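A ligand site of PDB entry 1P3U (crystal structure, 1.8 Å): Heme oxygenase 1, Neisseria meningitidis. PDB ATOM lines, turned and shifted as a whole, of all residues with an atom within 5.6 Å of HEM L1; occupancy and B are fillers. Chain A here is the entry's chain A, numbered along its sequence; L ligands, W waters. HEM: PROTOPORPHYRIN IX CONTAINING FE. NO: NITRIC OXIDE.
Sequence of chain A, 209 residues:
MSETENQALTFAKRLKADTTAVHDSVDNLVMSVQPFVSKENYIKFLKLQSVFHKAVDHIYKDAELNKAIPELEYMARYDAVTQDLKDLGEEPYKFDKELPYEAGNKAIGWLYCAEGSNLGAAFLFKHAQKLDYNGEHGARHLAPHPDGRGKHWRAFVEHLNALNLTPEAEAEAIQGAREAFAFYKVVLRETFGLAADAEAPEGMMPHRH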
ATOM      1  N   ALA A  12     -24.521 -20.279  -8.297  1.00  0.00           N
ATOM      2  CA  ALA A  12     -24.512 -18.875  -7.909  1.00  0.00           C
ATOM      3  C   ALA A  12     -23.810 -17.989  -8.933  1.00  0.00           C
ATOM      4  O   ALA A  12     -24.251 -16.860  -9.190  1.00  0.00           O
ATOM      5  CB  ALA A  12     -23.845 -18.719  -6.539  1.00  0.00           C
ATOM      6  N   LYS A  16     -25.382 -14.954 -11.307  1.00  0.00           N
ATOM      7  CA  LYS A  16     -24.758 -13.649 -11.423  1.00  0.00           C
ATOM      8  C   LYS A  16     -24.461 -13.303 -12.881  1.00  0.00           C
ATOM      9  O   LYS A  16     -24.867 -12.259 -13.378  1.00  0.00           O
ATOM     10  CB  LYS A  16     -23.472 -13.609 -10.602  1.00  0.00           C
ATOM     11  CG  LYS A  16     -22.692 -12.300 -10.702  1.00  0.00           C
ATOM     12  CD  LYS A  16     -21.537 -12.302  -9.718  1.00  0.00           C
ATOM     13  CE  LYS A  16     -20.607 -11.117  -9.930  1.00  0.00           C
ATOM     14  NZ  LYS A  16     -21.339  -9.824  -9.937  1.00  0.00           N
ATOM     15  N   HIS A  23     -29.092  -6.288 -13.641  1.00  0.00           N
ATOM     16  CA  HIS A  23     -28.795  -5.716 -12.336  1.00  0.00           C
ATOM     17  C   HIS A  23     -28.254  -4.306 -12.521  1.00  0.00           C
ATOM     18  O   HIS A  23     -28.676  -3.382 -11.832  1.00  0.00           O
ATOM     19  CB  HIS A  23     -27.741  -6.531 -11.592  1.00  0.00           C
ATOM     20  CG  HIS A  23     -27.206  -5.838 -10.376  1.00  0.00           C
ATOM     21  ND1 HIS A  23     -26.228  -4.868 -10.442  1.00  0.00           N
ATOM     22  CD2 HIS A  23     -27.567  -5.934  -9.078  1.00  0.00           C
ATOM     23  CE1 HIS A  23     -26.007  -4.401  -9.230  1.00  0.00           C
ATOM     24  NE2 HIS A  23     -26.808  -5.030  -8.377  1.00  0.00           N
ATOM     25  N   VAL A  26     -30.829  -1.868 -13.197  1.00  0.00           N
ATOM     26  CA  VAL A  26     -31.569  -1.497 -11.993  1.00  0.00           C
ATOM     27  C   VAL A  26     -30.774  -0.440 -11.225  1.00  0.00           C
ATOM     28  O   VAL A  26     -31.327   0.587 -10.833  1.00  0.00           O
ATOM     29  CB  VAL A  26     -31.818  -2.736 -11.103  1.00  0.00           C
ATOM     30  CG1 VAL A  26     -32.305  -2.307  -9.717  1.00  0.00           C
ATOM     31  CG2 VAL A  26     -32.833  -3.628 -11.771  1.00  0.00           C
ATOM     32  N   ASP A  27     -29.485  -0.702 -11.059  1.00  0.00           N
ATOM     33  CA  ASP A  27     -28.567   0.221 -10.380  1.00  0.00           C
ATOM     34  C   ASP A  27     -28.728   1.594 -11.035  1.00  0.00           C
ATOM     35  O   ASP A  27     -29.033   2.587 -10.369  1.00  0.00           O
ATOM     36  CB  ASP A  27     -27.121  -0.286 -10.590  1.00  0.00           C
ATOM     37  CG  ASP A  27     -26.056   0.622  -9.980  1.00  0.00           C
ATOM     38  OD1 ASP A  27     -26.305   1.838  -9.792  1.00  0.00           O
ATOM     39  OD2 ASP A  27     -24.948   0.114  -9.719  1.00  0.00           O
ATOM     40  N   ASN A  28     -28.569   1.637 -12.355  1.00  0.00           N
ATOM     41  CA  ASN A  28     -28.674   2.896 -13.087  1.00  0.00           C
ATOM     42  C   ASN A  28     -30.034   3.568 -12.938  1.00  0.00           C
ATOM     43  O   ASN A  28     -30.110   4.787 -12.747  1.00  0.00           O
ATOM     44  CB  ASN A  28     -28.373   2.684 -14.581  1.00  0.00           C
ATOM     45  CG  ASN A  28     -26.932   2.316 -14.845  1.00  0.00           C
ATOM     46  OD1 ASN A  28     -26.034   2.733 -14.116  1.00  0.00           O
ATOM     47  ND2 ASN A  28     -26.697   1.535 -15.903  1.00  0.00           N
ATOM     48  N   VAL A  30     -32.282   3.178 -10.459  1.00  0.00           N
ATOM     49  CA  VAL A  30     -32.429   3.647  -9.085  1.00  0.00           C
ATOM     50  C   VAL A  30     -31.695   4.981  -8.904  1.00  0.00           C
ATOM     51  O   VAL A  30     -32.249   5.948  -8.394  1.00  0.00           O
ATOM     52  CB  VAL A  30     -31.867   2.629  -8.075  1.00  0.00           C
ATOM     53  CG1 VAL A  30     -31.722   3.268  -6.685  1.00  0.00           C
ATOM     54  CG2 VAL A  30     -32.791   1.432  -8.005  1.00  0.00           C
ATOM     55  N   MET A  31     -30.438   5.033  -9.325  1.00  0.00           N
ATOM     56  CA  MET A  31     -29.690   6.267  -9.161  1.00  0.00           C
ATOM     57  C   MET A  31     -30.281   7.399 -10.008  1.00  0.00           C
ATOM     58  O   MET A  31     -30.309   8.544  -9.570  1.00  0.00           O
ATOM     59  CB  MET A  31     -28.219   6.034  -9.502  1.00  0.00           C
ATOM     60  CG  MET A  31     -27.523   5.057  -8.543  1.00  0.00           C
ATOM     61  SD  MET A  31     -27.772   5.461  -6.785  1.00  0.00           S
ATOM     62  CE  MET A  31     -26.687   6.886  -6.583  1.00  0.00           C
ATOM     63  N   GLN A  49     -38.817  -0.307  -1.933  1.00  0.00           N
ATOM     64  CA  GLN A  49     -38.166  -1.388  -1.208  1.00  0.00           C
ATOM     65  C   GLN A  49     -39.204  -2.211  -0.449  1.00  0.00           C
ATOM     66  O   GLN A  49     -39.135  -3.444  -0.408  1.00  0.00           O
ATOM     67  CB  GLN A  49     -37.131  -0.818  -0.227  1.00  0.00           C
ATOM     68  CG  GLN A  49     -35.935  -0.157  -0.903  1.00  0.00           C
ATOM     69  CD  GLN A  49     -34.909  -1.161  -1.387  1.00  0.00           C
ATOM     70  OE1 GLN A  49     -33.886  -1.411  -0.735  1.00  0.00           O
ATOM     71  NE2 GLN A  49     -35.177  -1.761  -2.542  1.00  0.00           N
ATOM     72  N   PHE A  52     -41.003  -4.688  -2.855  1.00  0.00           N
ATOM     73  CA  PHE A  52     -40.168  -5.812  -3.236  1.00  0.00           C
ATOM     74  C   PHE A  52     -39.943  -6.764  -2.084  1.00  0.00           C
ATOM     75  O   PHE A  52     -40.064  -7.975  -2.255  1.00  0.00           O
ATOM     76  CB  PHE A  52     -38.807  -5.332  -3.762  1.00  0.00           C
ATOM     77  CG  PHE A  52     -37.974  -6.436  -4.302  1.00  0.00           C
ATOM     78  CD1 PHE A  52     -38.313  -7.047  -5.505  1.00  0.00           C
ATOM     79  CD2 PHE A  52     -36.885  -6.926  -3.599  1.00  0.00           C
ATOM     80  CE1 PHE A  52     -37.577  -8.121  -6.000  1.00  0.00           C
ATOM     81  CE2 PHE A  52     -36.146  -8.009  -4.077  1.00  0.00           C
ATOM     82  CZ  PHE A  52     -36.493  -8.605  -5.282  1.00  0.00           C
ATOM     83  N   TYR A 112     -32.474 -15.237  -4.647  1.00  0.00           N
ATOM     84  CA  TYR A 112     -31.117 -14.828  -5.026  1.00  0.00           C
ATOM     85  C   TYR A 112     -31.087 -13.306  -5.216  1.00  0.00           C
ATOM     86  O   TYR A 112     -30.187 -12.616  -4.760  1.00  0.00           O
ATOM     87  CB  TYR A 112     -30.697 -15.507  -6.329  1.00  0.00           C
ATOM     88  CG  TYR A 112     -29.538 -14.819  -7.008  1.00  0.00           C
ATOM     89  CD1 TYR A 112     -28.240 -14.906  -6.499  1.00  0.00           C
ATOM     90  CD2 TYR A 112     -29.755 -14.010  -8.130  1.00  0.00           C
ATOM     91  CE1 TYR A 112     -27.194 -14.196  -7.077  1.00  0.00           C
ATOM     92  CE2 TYR A 112     -28.714 -13.304  -8.720  1.00  0.00           C
ATOM     93  CZ  TYR A 112     -27.434 -13.403  -8.191  1.00  0.00           C
ATOM     94  OH  TYR A 112     -26.406 -12.692  -8.755  1.00  0.00           O
ATOM     95  N   CYS A 113     -32.106 -12.812  -5.908  1.00  0.00           N
ATOM     96  CA  CYS A 113     -32.204 -11.388  -6.189  1.00  0.00           C
ATOM     97  C   CYS A 113     -32.269 -10.576  -4.889  1.00  0.00           C
ATOM     98  O   CYS A 113     -31.489  -9.641  -4.697  1.00  0.00           O
ATOM     99  CB  CYS A 113     -33.446 -11.123  -7.040  1.00  0.00           C
ATOM    100  SG  CYS A 113     -33.669  -9.417  -7.531  1.00  0.00           S
ATOM    101  N   ALA A 114     -33.176 -10.945  -3.991  1.00  0.00           N
ATOM    102  CA  ALA A 114     -33.343 -10.241  -2.724  1.00  0.00           C
ATOM    103  C   ALA A 114     -32.133 -10.314  -1.785  1.00  0.00           C
ATOM    104  O   ALA A 114     -31.772  -9.310  -1.162  1.00  0.00           O
ATOM    105  CB  ALA A 114     -34.583 -10.747  -1.997  1.00  0.00           C
ATOM    106  N   GLU A 115     -31.541 -11.490  -1.659  1.00  0.00           N
ATOM    107  CA  GLU A 115     -30.412 -11.663  -0.764  1.00  0.00           C
ATOM    108  C   GLU A 115     -29.153 -11.012  -1.334  1.00  0.00           C
ATOM    109  O   GLU A 115     -28.347 -10.451  -0.595  1.00  0.00           O
ATOM    110  CB  GLU A 115     -30.175 -13.155  -0.498  1.00  0.00           C
ATOM    111  CG  GLU A 115     -29.223 -13.434   0.673  1.00  0.00           C
ATOM    112  CD  GLU A 115     -29.578 -12.644   1.927  1.00  0.00           C
ATOM    113  OE1 GLU A 115     -30.777 -12.487   2.235  1.00  0.00           O
ATOM    114  OE2 GLU A 115     -28.639 -12.180   2.616  1.00  0.00           O
ATOM    115  N   GLY A 116     -28.999 -11.083  -2.651  1.00  0.00           N
ATOM    116  CA  GLY A 116     -27.843 -10.458  -3.258  1.00  0.00           C
ATOM    117  C   GLY A 116     -27.917  -8.953  -3.041  1.00  0.00           C
ATOM    118  O   GLY A 116     -26.896  -8.296  -2.862  1.00  0.00           O
ATOM    119  N   SER A 117     -29.128  -8.410  -3.074  1.00  0.00           N
ATOM    120  CA  SER A 117     -29.297  -6.963  -2.878  1.00  0.00           C
ATOM    121  C   SER A 117     -28.805  -6.561  -1.502  1.00  0.00           C
ATOM    122  O   SER A 117     -28.414  -5.414  -1.278  1.00  0.00           O
ATOM    123  CB  SER A 117     -30.774  -6.554  -3.038  1.00  0.00           C
ATOM    124  OG  SER A 117     -31.545  -6.918  -1.915  1.00  0.00           O
ATOM    125  N   LEU A 119     -26.190  -7.995  -0.029  1.00  0.00           N
ATOM    126  CA  LEU A 119     -24.743  -7.973  -0.162  1.00  0.00           C
ATOM    127  C   LEU A 119     -24.277  -6.647  -0.768  1.00  0.00           C
ATOM    128  O   LEU A 119     -23.355  -6.005  -0.272  1.00  0.00           O
ATOM    129  CB  LEU A 119     -24.268  -9.112  -1.068  1.00  0.00           C
ATOM    130  CG  LEU A 119     -22.812  -9.008  -1.546  1.00  0.00           C
ATOM    131  CD1 LEU A 119     -21.857  -9.335  -0.399  1.00  0.00           C
ATOM    132  CD2 LEU A 119     -22.583  -9.934  -2.718  1.00  0.00           C
ATOM    133  N   GLY A 120     -24.943  -6.236  -1.851  1.00  0.00           N
ATOM    134  CA  GLY A 120     -24.558  -5.007  -2.535  1.00  0.00           C
ATOM    135  C   GLY A 120     -25.132  -3.709  -2.006  1.00  0.00           C
ATOM    136  O   GLY A 120     -24.906  -2.645  -2.593  1.00  0.00           O
ATOM    137  N   ALA A 121     -25.853  -3.767  -0.891  1.00  0.00           N
ATOM    138  CA  ALA A 121     -26.471  -2.575  -0.315  1.00  0.00           C
ATOM    139  C   ALA A 121     -25.488  -1.587   0.315  1.00  0.00           C
ATOM    140  O   ALA A 121     -25.890  -0.541   0.800  1.00  0.00           O
ATOM    141  CB  ALA A 121     -27.517  -2.981   0.716  1.00  0.00           C
ATOM    142  N   PHE A 123     -23.334   0.458  -1.023  1.00  0.00           N
ATOM    143  CA  PHE A 123     -23.355   1.763  -1.693  1.00  0.00           C
ATOM    144  C   PHE A 123     -24.551   2.591  -1.240  1.00  0.00           C
ATOM    145  O   PHE A 123     -24.391   3.748  -0.832  1.00  0.00           O
ATOM    146  CB  PHE A 123     -23.409   1.577  -3.208  1.00  0.00           C
ATOM    147  CG  PHE A 123     -23.382   2.863  -3.986  1.00  0.00           C
ATOM    148  CD1 PHE A 123     -22.175   3.505  -4.267  1.00  0.00           C
ATOM    149  CD2 PHE A 123     -24.571   3.441  -4.424  1.00  0.00           C
ATOM    150  CE1 PHE A 123     -22.162   4.702  -4.985  1.00  0.00           C
ATOM    151  CE2 PHE A 123     -24.560   4.643  -5.150  1.00  0.00           C
ATOM    152  CZ  PHE A 123     -23.342   5.278  -5.426  1.00  0.00           C
ATOM    153  N   LEU A 124     -25.741   2.017  -1.302  1.00  0.00           N
ATOM    154  CA  LEU A 124     -26.943   2.720  -0.874  1.00  0.00           C
ATOM    155  C   LEU A 124     -26.847   3.155   0.583  1.00  0.00           C
ATOM    156  O   LEU A 124     -27.276   4.253   0.941  1.00  0.00           O
ATOM    157  CB  LEU A 124     -28.173   1.838  -1.067  1.00  0.00           C
ATOM    158  CG  LEU A 124     -28.532   1.540  -2.509  1.00  0.00           C
ATOM    159  CD1 LEU A 124     -29.677   0.507  -2.554  1.00  0.00           C
ATOM    160  CD2 LEU A 124     -28.959   2.831  -3.197  1.00  0.00           C
ATOM    161  N   TRP A 153     -22.948 -13.450   3.068  1.00  0.00           N
ATOM    162  CA  TRP A 153     -23.272 -13.824   1.695  1.00  0.00           C
ATOM    163  C   TRP A 153     -22.606 -15.140   1.264  1.00  0.00           C
ATOM    164  O   TRP A 153     -23.255 -16.009   0.684  1.00  0.00           O
ATOM    165  CB  TRP A 153     -22.858 -12.680   0.750  1.00  0.00           C
ATOM    166  CG  TRP A 153     -22.979 -12.991  -0.710  1.00  0.00           C
ATOM    167  CD1 TRP A 153     -21.948 -13.094  -1.603  1.00  0.00           C
ATOM    168  CD2 TRP A 153     -24.186 -13.190  -1.466  1.00  0.00           C
ATOM    169  NE1 TRP A 153     -22.443 -13.335  -2.867  1.00  0.00           N
ATOM    170  CE2 TRP A 153     -23.804 -13.391  -2.812  1.00  0.00           C
ATOM    171  CE3 TRP A 153     -25.547 -13.202  -1.131  1.00  0.00           C
ATOM    172  CZ2 TRP A 153     -24.743 -13.617  -3.825  1.00  0.00           C
ATOM    173  CZ3 TRP A 153     -26.473 -13.422  -2.143  1.00  0.00           C
ATOM    174  CH2 TRP A 153     -26.066 -13.627  -3.473  1.00  0.00           C
ATOM    175  N   PHE A 181     -35.904  -8.976 -10.950  1.00  0.00           N
ATOM    176  CA  PHE A 181     -35.319  -7.678 -11.289  1.00  0.00           C
ATOM    177  C   PHE A 181     -36.315  -6.889 -12.135  1.00  0.00           C
ATOM    178  O   PHE A 181     -36.455  -5.680 -11.970  1.00  0.00           O
ATOM    179  CB  PHE A 181     -34.020  -7.866 -12.082  1.00  0.00           C
ATOM    180  CG  PHE A 181     -32.801  -8.131 -11.238  1.00  0.00           C
ATOM    181  CD1 PHE A 181     -32.099  -9.336 -11.362  1.00  0.00           C
ATOM    182  CD2 PHE A 181     -32.327  -7.174 -10.355  1.00  0.00           C
ATOM    183  CE1 PHE A 181     -30.946  -9.570 -10.615  1.00  0.00           C
ATOM    184  CE2 PHE A 181     -31.171  -7.400  -9.605  1.00  0.00           C
ATOM    185  CZ  PHE A 181     -30.471  -8.600  -9.737  1.00  0.00           C
ATOM    186  N   TYR A 184     -38.924  -5.415  -9.988  1.00  0.00           N
ATOM    187  CA  TYR A 184     -38.377  -4.292  -9.242  1.00  0.00           C
ATOM    188  C   TYR A 184     -38.504  -3.011 -10.061  1.00  0.00           C
ATOM    189  O   TYR A 184     -38.986  -1.997  -9.565  1.00  0.00           O
ATOM    190  CB  TYR A 184     -36.895  -4.531  -8.887  1.00  0.00           C
ATOM    191  CG  TYR A 184     -36.362  -3.549  -7.869  1.00  0.00           C
ATOM    192  CD1 TYR A 184     -36.550  -3.757  -6.511  1.00  0.00           C
ATOM    193  CD2 TYR A 184     -35.700  -2.379  -8.273  1.00  0.00           C
ATOM    194  CE1 TYR A 184     -36.077  -2.837  -5.568  1.00  0.00           C
ATOM    195  CE2 TYR A 184     -35.232  -1.463  -7.342  1.00  0.00           C
ATOM    196  CZ  TYR A 184     -35.420  -1.700  -5.998  1.00  0.00           C
ATOM    197  OH  TYR A 184     -34.938  -0.793  -5.085  1.00  0.00           O
HETATM  198  CHA HEM L   1     -24.590  -7.190  -5.849  1.00  0.00           C
HETATM  199  CHB HEM L   1     -24.460  -2.391  -6.439  1.00  0.00           C
HETATM  200  CHC HEM L   1     -29.318  -2.290  -6.311  1.00  0.00           C
HETATM  201  CHD HEM L   1     -29.423  -7.123  -6.375  1.00  0.00           C
HETATM  202  C1A HEM L   1     -24.145  -5.883  -5.920  1.00  0.00           C
HETATM  203  C2A HEM L   1     -22.720  -5.502  -5.851  1.00  0.00           C
HETATM  204  C3A HEM L   1     -22.703  -4.168  -6.074  1.00  0.00           C
HETATM  205  C4A HEM L   1     -24.080  -3.719  -6.256  1.00  0.00           C
HETATM  206  CMA HEM L   1     -21.428  -3.353  -6.171  1.00  0.00           C
HETATM  207  CAA HEM L   1     -21.548  -6.434  -5.537  1.00  0.00           C
HETATM  208  CBA HEM L   1     -21.186  -6.391  -4.062  1.00  0.00           C
HETATM  209  CGA HEM L   1     -20.099  -7.379  -3.703  1.00  0.00           C
HETATM  210  O1A HEM L   1     -19.577  -7.300  -2.568  1.00  0.00           O
HETATM  211  O2A HEM L   1     -19.764  -8.240  -4.548  1.00  0.00           O
HETATM  212  C1B HEM L   1     -25.797  -1.968  -6.539  1.00  0.00           C
HETATM  213  C2B HEM L   1     -26.192  -0.569  -6.550  1.00  0.00           C
HETATM  214  C3B HEM L   1     -27.549  -0.513  -6.464  1.00  0.00           C
HETATM  215  C4B HEM L   1     -27.974  -1.920  -6.390  1.00  0.00           C
HETATM  216  CMB HEM L   1     -25.228   0.610  -6.613  1.00  0.00           C
HETATM  217  CAB HEM L   1     -28.417   0.590  -6.414  1.00  0.00           C
HETATM  218  CBB HEM L   1     -28.201   1.889  -7.008  1.00  0.00           C
HETATM  219  C1C HEM L   1     -29.765  -3.603  -6.277  1.00  0.00           C
HETATM  220  C2C HEM L   1     -31.165  -3.979  -6.269  1.00  0.00           C
HETATM  221  C3C HEM L   1     -31.214  -5.339  -6.369  1.00  0.00           C
HETATM  222  C4C HEM L   1     -29.815  -5.779  -6.367  1.00  0.00           C
HETATM  223  CMC HEM L   1     -32.344  -3.020  -6.038  1.00  0.00           C
HETATM  224  CAC HEM L   1     -32.318  -6.181  -6.498  1.00  0.00           C
HETATM  225  CBC HEM L   1     -33.710  -5.909  -6.211  1.00  0.00           C
HETATM  226  C1D HEM L   1     -28.087  -7.575  -6.288  1.00  0.00           C
HETATM  227  C2D HEM L   1     -27.672  -8.968  -6.392  1.00  0.00           C
HETATM  228  C3D HEM L   1     -26.328  -8.983  -6.207  1.00  0.00           C
HETATM  229  C4D HEM L   1     -25.915  -7.596  -6.029  1.00  0.00           C
HETATM  230  CMD HEM L   1     -28.571 -10.167  -6.588  1.00  0.00           C
HETATM  231  CAD HEM L   1     -25.482 -10.248  -6.094  1.00  0.00           C
HETATM  232  CBD HEM L   1     -24.465 -10.392  -7.207  1.00  0.00           C
HETATM  233  CGD HEM L   1     -23.660 -11.659  -7.054  1.00  0.00           C
HETATM  234  O1D HEM L   1     -24.194 -12.750  -7.369  1.00  0.00           O
HETATM  235  O2D HEM L   1     -22.492 -11.562  -6.622  1.00  0.00           O
HETATM  236  NA  HEM L   1     -24.956  -4.796  -6.160  1.00  0.00           N
HETATM  237  NB  HEM L   1     -26.902  -2.801  -6.439  1.00  0.00           N
HETATM  238  NC  HEM L   1     -28.940  -4.701  -6.327  1.00  0.00           N
HETATM  239  ND  HEM L   1     -26.989  -6.740  -6.139  1.00  0.00           N
HETATM  240 FE   HEM L   1     -26.949  -4.766  -6.269  1.00  0.00          FE
HETATM  241  N    NO L   2     -27.018  -4.472  -4.712  1.00  0.00           N
HETATM  242  O    NO L   2     -27.485  -3.837  -3.839  1.00  0.00           O
HETATM  243  O   HOH W   1     -20.675  -9.505  -6.806  1.00  0.00           O
HETATM  244  O   HOH W   2     -21.024  -7.615  -8.674  1.00  0.00           O
HETATM  245  O   HOH W   3     -20.624  -5.599  -0.658  1.00  0.00           O
HETATM  246  O   HOH W   4     -23.926  -6.814  -9.057  1.00  0.00           O
HETATM  247  O   HOH W   5     -28.417  -2.632  -9.405  1.00  0.00           O
HETATM  248  O   HOH W   6     -20.746 -13.145  -5.337  1.00  0.00           O
HETATM  249  O   HOH W   7     -23.170 -15.183  -7.193  1.00  0.00           O
HETATM  250  O   HOH W   8     -17.859  -9.035  -1.498  1.00  0.00           O
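The side-chain hydroxyl (OH) of Tyr 112 lies within hydrogen-bond range of an oxygen (O1D) of HEM L1 (2.6 Å).
The backbone NH (N) of Ala 121 sits at hydrogen-bond distance from an oxygen (O) of NO L2, at 3.4 Å.
NE2 of His 23 binds FE of HEM L1 (2.1 Å).
The side-chain amino group of Lys 16 lies within salt-bridge range of an oxygen (O2D) of HEM L1, 3.9 Å away.
A nitrogen (N) of NO L2 is bound to an iron atom (FE) of HEM L1 (1.6 Å).
The backbone carbonyl oxygen (O) of Ala 114 sits at hydrogen-bond distance from the side-chain hydroxyl (OG) of Ser 117.
OH of Tyr 184 sits at hydrogen-bond distance from NE2 of Gln 49 (2.7 Å).
Val 26 touches HEM L1 (CG1 to CMC, 3.7 Å).
Asp 27 touches HEM L1 (OD2 to CMB, 3.2 Å).
CG1 of Val 30 touches CBB of HEM L1, 3.8 Å away.
CG of Met 31 touches CBB of HEM L1, at 3.6 Å.
CE2 of Phe 52 touches CBC of HEM L1, 3.9 Å away.
Cys 113 touches HEM L1.
Gly 116 touches HEM L1 (C to C2D, 3.4 Å).
N of Ser 117 touches C1D of HEM L1, 3.5 Å away.
Leu 119 touches HEM L1.
CA of Gly 120 touches C1A of HEM L1, at 3.5 Å.
Phe 123 touches HEM L1.
Leu 124 touches HEM L1.
CZ2 of Trp 153 touches O1D of HEM L1, at 3.7 Å.
Phe 181 touches HEM L1.
Tyr 184 touches HEM L1.
Hydrophobic or aromatic side chains that line HEM L1: His 23, Val 26, Val 30, Met 31, Phe 52, Tyr 112, Leu 119, Phe 123, Leu 124, Trp 153, Phe 181 and Tyr 184.
The nearest printed residue that does not touch HEM L1 is Ala 12 (4.5 Å).
Water W7 lies within hydrogen-bond range of O1D of HEM L1 and O of Ala 12.
Water W6 lies within hydrogen-bond range of an oxygen (O2D) of HEM L1 (2.7 Å) and the indole nitrogen of Trp 153 (3.0 Å).
Water W1 bridges an oxygen (O2A) of HEM L1 and the side-chain amino group (NZ) of Lys 16.
Water W3 lies within hydrogen-bond range of an oxygen (O1A) of HEM L1 (2.8 Å) and the backbone carbonyl oxygen (O) of Leu 119 (2.8 Å).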
